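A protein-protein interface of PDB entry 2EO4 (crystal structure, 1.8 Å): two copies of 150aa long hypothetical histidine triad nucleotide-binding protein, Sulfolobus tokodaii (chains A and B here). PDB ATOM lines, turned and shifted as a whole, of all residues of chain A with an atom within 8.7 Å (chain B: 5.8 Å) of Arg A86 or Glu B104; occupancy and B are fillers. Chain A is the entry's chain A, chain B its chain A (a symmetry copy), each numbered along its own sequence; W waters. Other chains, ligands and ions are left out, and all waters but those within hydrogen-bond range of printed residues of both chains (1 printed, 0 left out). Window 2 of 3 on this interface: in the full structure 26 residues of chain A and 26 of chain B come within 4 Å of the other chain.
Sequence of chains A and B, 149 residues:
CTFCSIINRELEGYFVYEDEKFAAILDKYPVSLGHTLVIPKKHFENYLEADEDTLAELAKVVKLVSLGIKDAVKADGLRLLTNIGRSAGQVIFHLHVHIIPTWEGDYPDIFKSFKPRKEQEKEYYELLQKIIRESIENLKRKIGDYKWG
The backbone NH of Ala A88 lies within hydrogen-bond range of the side-chain hydroxyl of Thr B102 (3.5 Å).
The side-chain hydroxyl (OG1) of Thr B102 sits at hydrogen-bond distance from the side-chain hydroxyl (OG) of Ser A87.
The side-chain carboxylate (OE1) of Glu B104 lies within salt-bridge range of the guanidinium group (NH2) of Arg A86 (2.7 Å).
The backbone carbonyl oxygen of Thr B102 sits at hydrogen-bond distance from the backbone NH of Asp B76, 3.0 Å away.
The side-chain amide oxygen (OD1) of Asn A83 lies close to the backbone carbonyl oxygen (O) of Ala A88 (3.1 Å).
OD2 of Asp B76 is in hydrogen-bond range of N of Glu B104 (2.9 Å).
Asp B76 touches Ser A87.
Trp B103 touches Ser A87.
Glu B104 touches Ser A87 (CG to CB, 3.8 Å).
Of the printed residues of chain B, Ser A87 touches Asp B76 (3.7 Å), Thr B102 (2.8 Å), Trp B103 (3.8 Å) and Glu B104 (3.8 Å).
Printed residues of chain B within 4 Å of Ala A88: Thr B102.
Of the printed residues of chain A, Thr B102 touches Ser A87 (2.8 Å) and Ala A88 (3.5 Å).
Printed residues of chain A within 4 Å of Trp B103: Ser A87 (3.8 Å).
Glu B104 touches two residues of chain A.
The nearest residue of chain B that does not touch Arg A86 is Asp B76 (5.5 Å).
The nearest residue of chain A that does not touch Glu B104 is Gly A85 (6.2 Å).
Printed residues of chain B that touch a printed residue of chain A: Asp B76, Thr B102, Trp B103 and Glu B104.
Printed residues of chain A that touch a printed residue of chain B: Arg A86, Ser A87 and Ala A88.
Among the printed residues, Asp or Glu carboxylates within 4 Å of a Lys or Arg side-chain nitrogen of the other chain: Arg A86 with Glu B104 (2.7 Å).
No position is printed for both chains.
Of the 6 pairs that touch across the chains among the printed residues, none has its exchanged pair printed and touching as well.
Water W1 lies within hydrogen-bond range of OG of Ser A87 (2.8 Å), OE2 of Glu B104 (2.9 Å), O of Asp B76 (3.2 Å) and N of Arg A86 (3.4 Å).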
ATOM      1  N   ASN A  46      15.319   1.858  22.035  1.00  0.00           N
ATOM      2  CA  ASN A  46      16.595   1.183  22.225  1.00  0.00           C
ATOM      3  C   ASN A  46      17.703   2.209  22.437  1.00  0.00           C
ATOM      4  O   ASN A  46      17.447   3.412  22.489  1.00  0.00           O
ATOM      5  CB  ASN A  46      16.908   0.309  21.006  1.00  0.00           C
ATOM      6  CG  ASN A  46      16.940   1.107  19.715  1.00  0.00           C
ATOM      7  OD1 ASN A  46      17.718   2.048  19.580  1.00  0.00           O
ATOM      8  ND2 ASN A  46      16.090   0.734  18.759  1.00  0.00           N
ATOM      9  N   ASN A  83      20.598  -4.740  24.171  1.00  0.00           N
ATOM     10  CA  ASN A  83      20.269  -5.263  22.854  1.00  0.00           C
ATOM     11  C   ASN A  83      19.427  -4.308  22.037  1.00  0.00           C
ATOM     12  O   ASN A  83      18.522  -3.661  22.559  1.00  0.00           O
ATOM     13  CB  ASN A  83      19.535  -6.592  23.010  1.00  0.00           C
ATOM     14  CG  ASN A  83      20.351  -7.610  23.764  1.00  0.00           C
ATOM     15  OD1 ASN A  83      21.500  -7.874  23.412  1.00  0.00           O
ATOM     16  ND2 ASN A  83      19.761  -8.199  24.807  1.00  0.00           N
ATOM     17  N   ILE A  84      19.733  -4.232  20.746  1.00  0.00           N
ATOM     18  CA  ILE A  84      19.013  -3.356  19.830  1.00  0.00           C
ATOM     19  C   ILE A  84      18.414  -4.210  18.719  1.00  0.00           C
ATOM     20  O   ILE A  84      19.137  -4.709  17.863  1.00  0.00           O
ATOM     21  CB  ILE A  84      19.965  -2.321  19.198  1.00  0.00           C
ATOM     22  CG1 ILE A  84      20.611  -1.468  20.294  1.00  0.00           C
ATOM     23  CG2 ILE A  84      19.197  -1.435  18.226  1.00  0.00           C
ATOM     24  CD1 ILE A  84      21.874  -0.742  19.832  1.00  0.00           C
ATOM     25  N   GLY A  85      17.098  -4.385  18.749  1.00  0.00           N
ATOM     26  CA  GLY A  85      16.437  -5.182  17.726  1.00  0.00           C
ATOM     27  C   GLY A  85      16.176  -6.615  18.149  1.00  0.00           C
ATOM     28  O   GLY A  85      16.947  -7.206  18.912  1.00  0.00           O
ATOM     29  N   ARG A  86      15.089  -7.193  17.646  1.00  0.00           N
ATOM     30  CA  ARG A  86      14.754  -8.564  17.999  1.00  0.00           C
ATOM     31  C   ARG A  86      15.826  -9.568  17.582  1.00  0.00           C
ATOM     32  O   ARG A  86      16.043 -10.556  18.283  1.00  0.00           O
ATOM     33  CB  ARG A  86      13.398  -8.957  17.397  1.00  0.00           C
ATOM     34  CG  ARG A  86      13.342  -8.913  15.884  1.00  0.00           C
ATOM     35  CD  ARG A  86      11.968  -9.350  15.392  1.00  0.00           C
ATOM     36  NE  ARG A  86      11.872  -9.304  13.936  1.00  0.00           N
ATOM     37  CZ  ARG A  86      10.800  -9.683  13.246  1.00  0.00           C
ATOM     38  NH1 ARG A  86       9.727 -10.142  13.878  1.00  0.00           N
ATOM     39  NH2 ARG A  86      10.803  -9.600  11.922  1.00  0.00           N
ATOM     40  N   SER A  87      16.510  -9.322  16.464  1.00  0.00           N
ATOM     41  CA  SER A  87      17.545 -10.253  16.016  1.00  0.00           C
ATOM     42  C   SER A  87      18.776 -10.228  16.921  1.00  0.00           C
ATOM     43  O   SER A  87      19.639 -11.097  16.827  1.00  0.00           O
ATOM     44  CB  SER A  87      17.955  -9.980  14.556  1.00  0.00           C
ATOM     45  OG  SER A  87      18.558  -8.707  14.379  1.00  0.00           O
ATOM     46  N   ALA A  88      18.845  -9.237  17.804  1.00  0.00           N
ATOM     47  CA  ALA A  88      19.960  -9.132  18.740  1.00  0.00           C
ATOM     48  C   ALA A  88      19.496  -9.605  20.115  1.00  0.00           C
ATOM     49  O   ALA A  88      20.234  -9.512  21.095  1.00  0.00           O
ATOM     50  CB  ALA A  88      20.456  -7.688  18.822  1.00  0.00           C
ATOM     51  N   GLY A  89      18.262 -10.101  20.181  1.00  0.00           N
ATOM     52  CA  GLY A  89      17.732 -10.597  21.438  1.00  0.00           C
ATOM     53  C   GLY A  89      16.883  -9.631  22.247  1.00  0.00           C
ATOM     54  O   GLY A  89      16.522  -9.936  23.384  1.00  0.00           O
ATOM     55  N   GLN A  90      16.562  -8.469  21.690  1.00  0.00           N
ATOM     56  CA  GLN A  90      15.737  -7.522  22.427  1.00  0.00           C
ATOM     57  C   GLN A  90      14.274  -7.966  22.412  1.00  0.00           C
ATOM     58  O   GLN A  90      13.741  -8.329  21.361  1.00  0.00           O
ATOM     59  CB  GLN A  90      15.861  -6.113  21.837  1.00  0.00           C
ATOM     60  CG  GLN A  90      14.979  -5.096  22.555  1.00  0.00           C
ATOM     61  CD  GLN A  90      15.211  -3.666  22.104  1.00  0.00           C
ATOM     62  OE1 GLN A  90      15.453  -3.402  20.925  1.00  0.00           O
ATOM     63  NE2 GLN A  90      15.115  -2.731  23.044  1.00  0.00           N
ATOM     64  N   VAL A  91      13.638  -7.950  23.582  1.00  0.00           N
ATOM     65  CA  VAL A  91      12.234  -8.339  23.707  1.00  0.00           C
ATOM     66  C   VAL A  91      11.420  -7.270  24.433  1.00  0.00           C
ATOM     67  O   VAL A  91      10.195  -7.228  24.310  1.00  0.00           O
ATOM     68  CB  VAL A  91      12.071  -9.700  24.439  1.00  0.00           C
ATOM     69  CG1 VAL A  91      12.754 -10.795  23.643  1.00  0.00           C
ATOM     70  CG2 VAL A  91      12.630  -9.618  25.850  1.00  0.00           C
ATOM     71  N   ILE A  92      12.089  -6.423  25.213  1.00  0.00           N
ATOM     72  CA  ILE A  92      11.401  -5.325  25.891  1.00  0.00           C
ATOM     73  C   ILE A  92      11.931  -4.073  25.206  1.00  0.00           C
ATOM     74  O   ILE A  92      13.113  -3.737  25.321  1.00  0.00           O
ATOM     75  CB  ILE A  92      11.710  -5.254  27.404  1.00  0.00           C
ATOM     76  CG1 ILE A  92      11.278  -6.551  28.093  1.00  0.00           C
ATOM     77  CG2 ILE A  92      10.957  -4.077  28.022  1.00  0.00           C
ATOM     78  CD1 ILE A  92      11.524  -6.566  29.596  1.00  0.00           C
ATOM     79  N   PHE A  93      11.055  -3.387  24.484  1.00  0.00           N
ATOM     80  CA  PHE A  93      11.468  -2.215  23.735  1.00  0.00           C
ATOM     81  C   PHE A  93      11.431  -0.885  24.466  1.00  0.00           C
ATOM     82  O   PHE A  93      10.763   0.069  24.061  1.00  0.00           O
ATOM     83  CB  PHE A  93      10.685  -2.192  22.422  1.00  0.00           C
ATOM     84  CG  PHE A  93      10.957  -3.400  21.574  1.00  0.00           C
ATOM     85  CD1 PHE A  93      12.089  -3.456  20.767  1.00  0.00           C
ATOM     86  CD2 PHE A  93      10.156  -4.534  21.679  1.00  0.00           C
ATOM     87  CE1 PHE A  93      12.426  -4.621  20.086  1.00  0.00           C
ATOM     88  CE2 PHE A  93      10.486  -5.706  21.002  1.00  0.00           C
ATOM     89  CZ  PHE A  93      11.625  -5.749  20.205  1.00  0.00           C
ATOM     90  N   ASP B  76      20.031  -5.579  11.072  1.00  0.00           N
ATOM     91  CA  ASP B  76      18.677  -5.430  11.583  1.00  0.00           C
ATOM     92  C   ASP B  76      18.753  -5.166  13.079  1.00  0.00           C
ATOM     93  O   ASP B  76      17.819  -4.636  13.680  1.00  0.00           O
ATOM     94  CB  ASP B  76      17.867  -6.695  11.321  1.00  0.00           C
ATOM     95  CG  ASP B  76      17.633  -6.925   9.845  1.00  0.00           C
ATOM     96  OD1 ASP B  76      17.146  -5.982   9.187  1.00  0.00           O
ATOM     97  OD2 ASP B  76      17.937  -8.029   9.353  1.00  0.00           O
ATOM     98  N   THR B 102      23.729  -7.997  13.940  1.00  0.00           N
ATOM     99  CA  THR B 102      22.871  -9.160  13.765  1.00  0.00           C
ATOM    100  C   THR B 102      21.911  -8.893  12.609  1.00  0.00           C
ATOM    101  O   THR B 102      21.683  -7.741  12.235  1.00  0.00           O
ATOM    102  CB  THR B 102      22.049  -9.473  15.042  1.00  0.00           C
ATOM    103  OG1 THR B 102      21.169  -8.381  15.339  1.00  0.00           O
ATOM    104  CG2 THR B 102      22.975  -9.707  16.227  1.00  0.00           C
ATOM    105  N   TRP B 103      21.363  -9.965  12.049  1.00  0.00           N
ATOM    106  CA  TRP B 103      20.419  -9.865  10.939  1.00  0.00           C
ATOM    107  C   TRP B 103      19.313 -10.882  11.156  1.00  0.00           C
ATOM    108  O   TRP B 103      19.537 -11.937  11.749  1.00  0.00           O
ATOM    109  CB  TRP B 103      21.115 -10.179   9.610  1.00  0.00           C
ATOM    110  CG  TRP B 103      22.187  -9.209   9.235  1.00  0.00           C
ATOM    111  CD1 TRP B 103      22.053  -8.098   8.450  1.00  0.00           C
ATOM    112  CD2 TRP B 103      23.555  -9.245   9.652  1.00  0.00           C
ATOM    113  NE1 TRP B 103      23.257  -7.441   8.353  1.00  0.00           N
ATOM    114  CE2 TRP B 103      24.195  -8.123   9.081  1.00  0.00           C
ATOM    115  CE3 TRP B 103      24.303 -10.118  10.453  1.00  0.00           C
ATOM    116  CZ2 TRP B 103      25.550  -7.850   9.288  1.00  0.00           C
ATOM    117  CZ3 TRP B 103      25.653  -9.844  10.659  1.00  0.00           C
ATOM    118  CH2 TRP B 103      26.259  -8.719  10.077  1.00  0.00           C
ATOM    119  N   GLU B 104      18.117 -10.570  10.677  1.00  0.00           N
ATOM    120  CA  GLU B 104      17.011 -11.498  10.818  1.00  0.00           C
ATOM    121  C   GLU B 104      17.186 -12.603   9.783  1.00  0.00           C
ATOM    122  O   GLU B 104      16.682 -13.712   9.945  1.00  0.00           O
ATOM    123  CB  GLU B 104      15.682 -10.761  10.645  1.00  0.00           C
ATOM    124  CG  GLU B 104      15.185 -10.159  11.954  1.00  0.00           C
ATOM    125  CD  GLU B 104      14.142  -9.084  11.762  1.00  0.00           C
ATOM    126  OE1 GLU B 104      13.245  -9.270  10.914  1.00  0.00           O
ATOM    127  OE2 GLU B 104      14.213  -8.055  12.469  1.00  0.00           O
ATOM    128  N   GLY B 105      17.932 -12.292   8.728  1.00  0.00           N
ATOM    129  CA  GLY B 105      18.197 -13.261   7.682  1.00  0.00           C
ATOM    130  C   GLY B 105      19.693 -13.468   7.527  1.00  0.00           C
ATOM    131  O   GLY B 105      20.343 -14.030   8.409  1.00  0.00           O
ATOM    132  N   ASP B 106      20.239 -13.009   6.404  1.00  0.00           N
ATOM    133  CA  ASP B 106      21.668 -13.127   6.127  1.00  0.00           C
ATOM    134  C   ASP B 106      22.223 -11.741   5.816  1.00  0.00           C
ATOM    135  O   ASP B 106      21.477 -10.850   5.409  1.00  0.00           O
ATOM    136  CB  ASP B 106      21.905 -14.052   4.929  1.00  0.00           C
ATOM    137  CG  ASP B 106      21.374 -15.454   5.159  1.00  0.00           C
ATOM    138  OD1 ASP B 106      21.851 -16.126   6.098  1.00  0.00           O
ATOM    139  OD2 ASP B 106      20.481 -15.885   4.399  1.00  0.00           O
HETATM  140  O   HOH W   1      16.178  -7.287  14.407  1.00  0.00           O
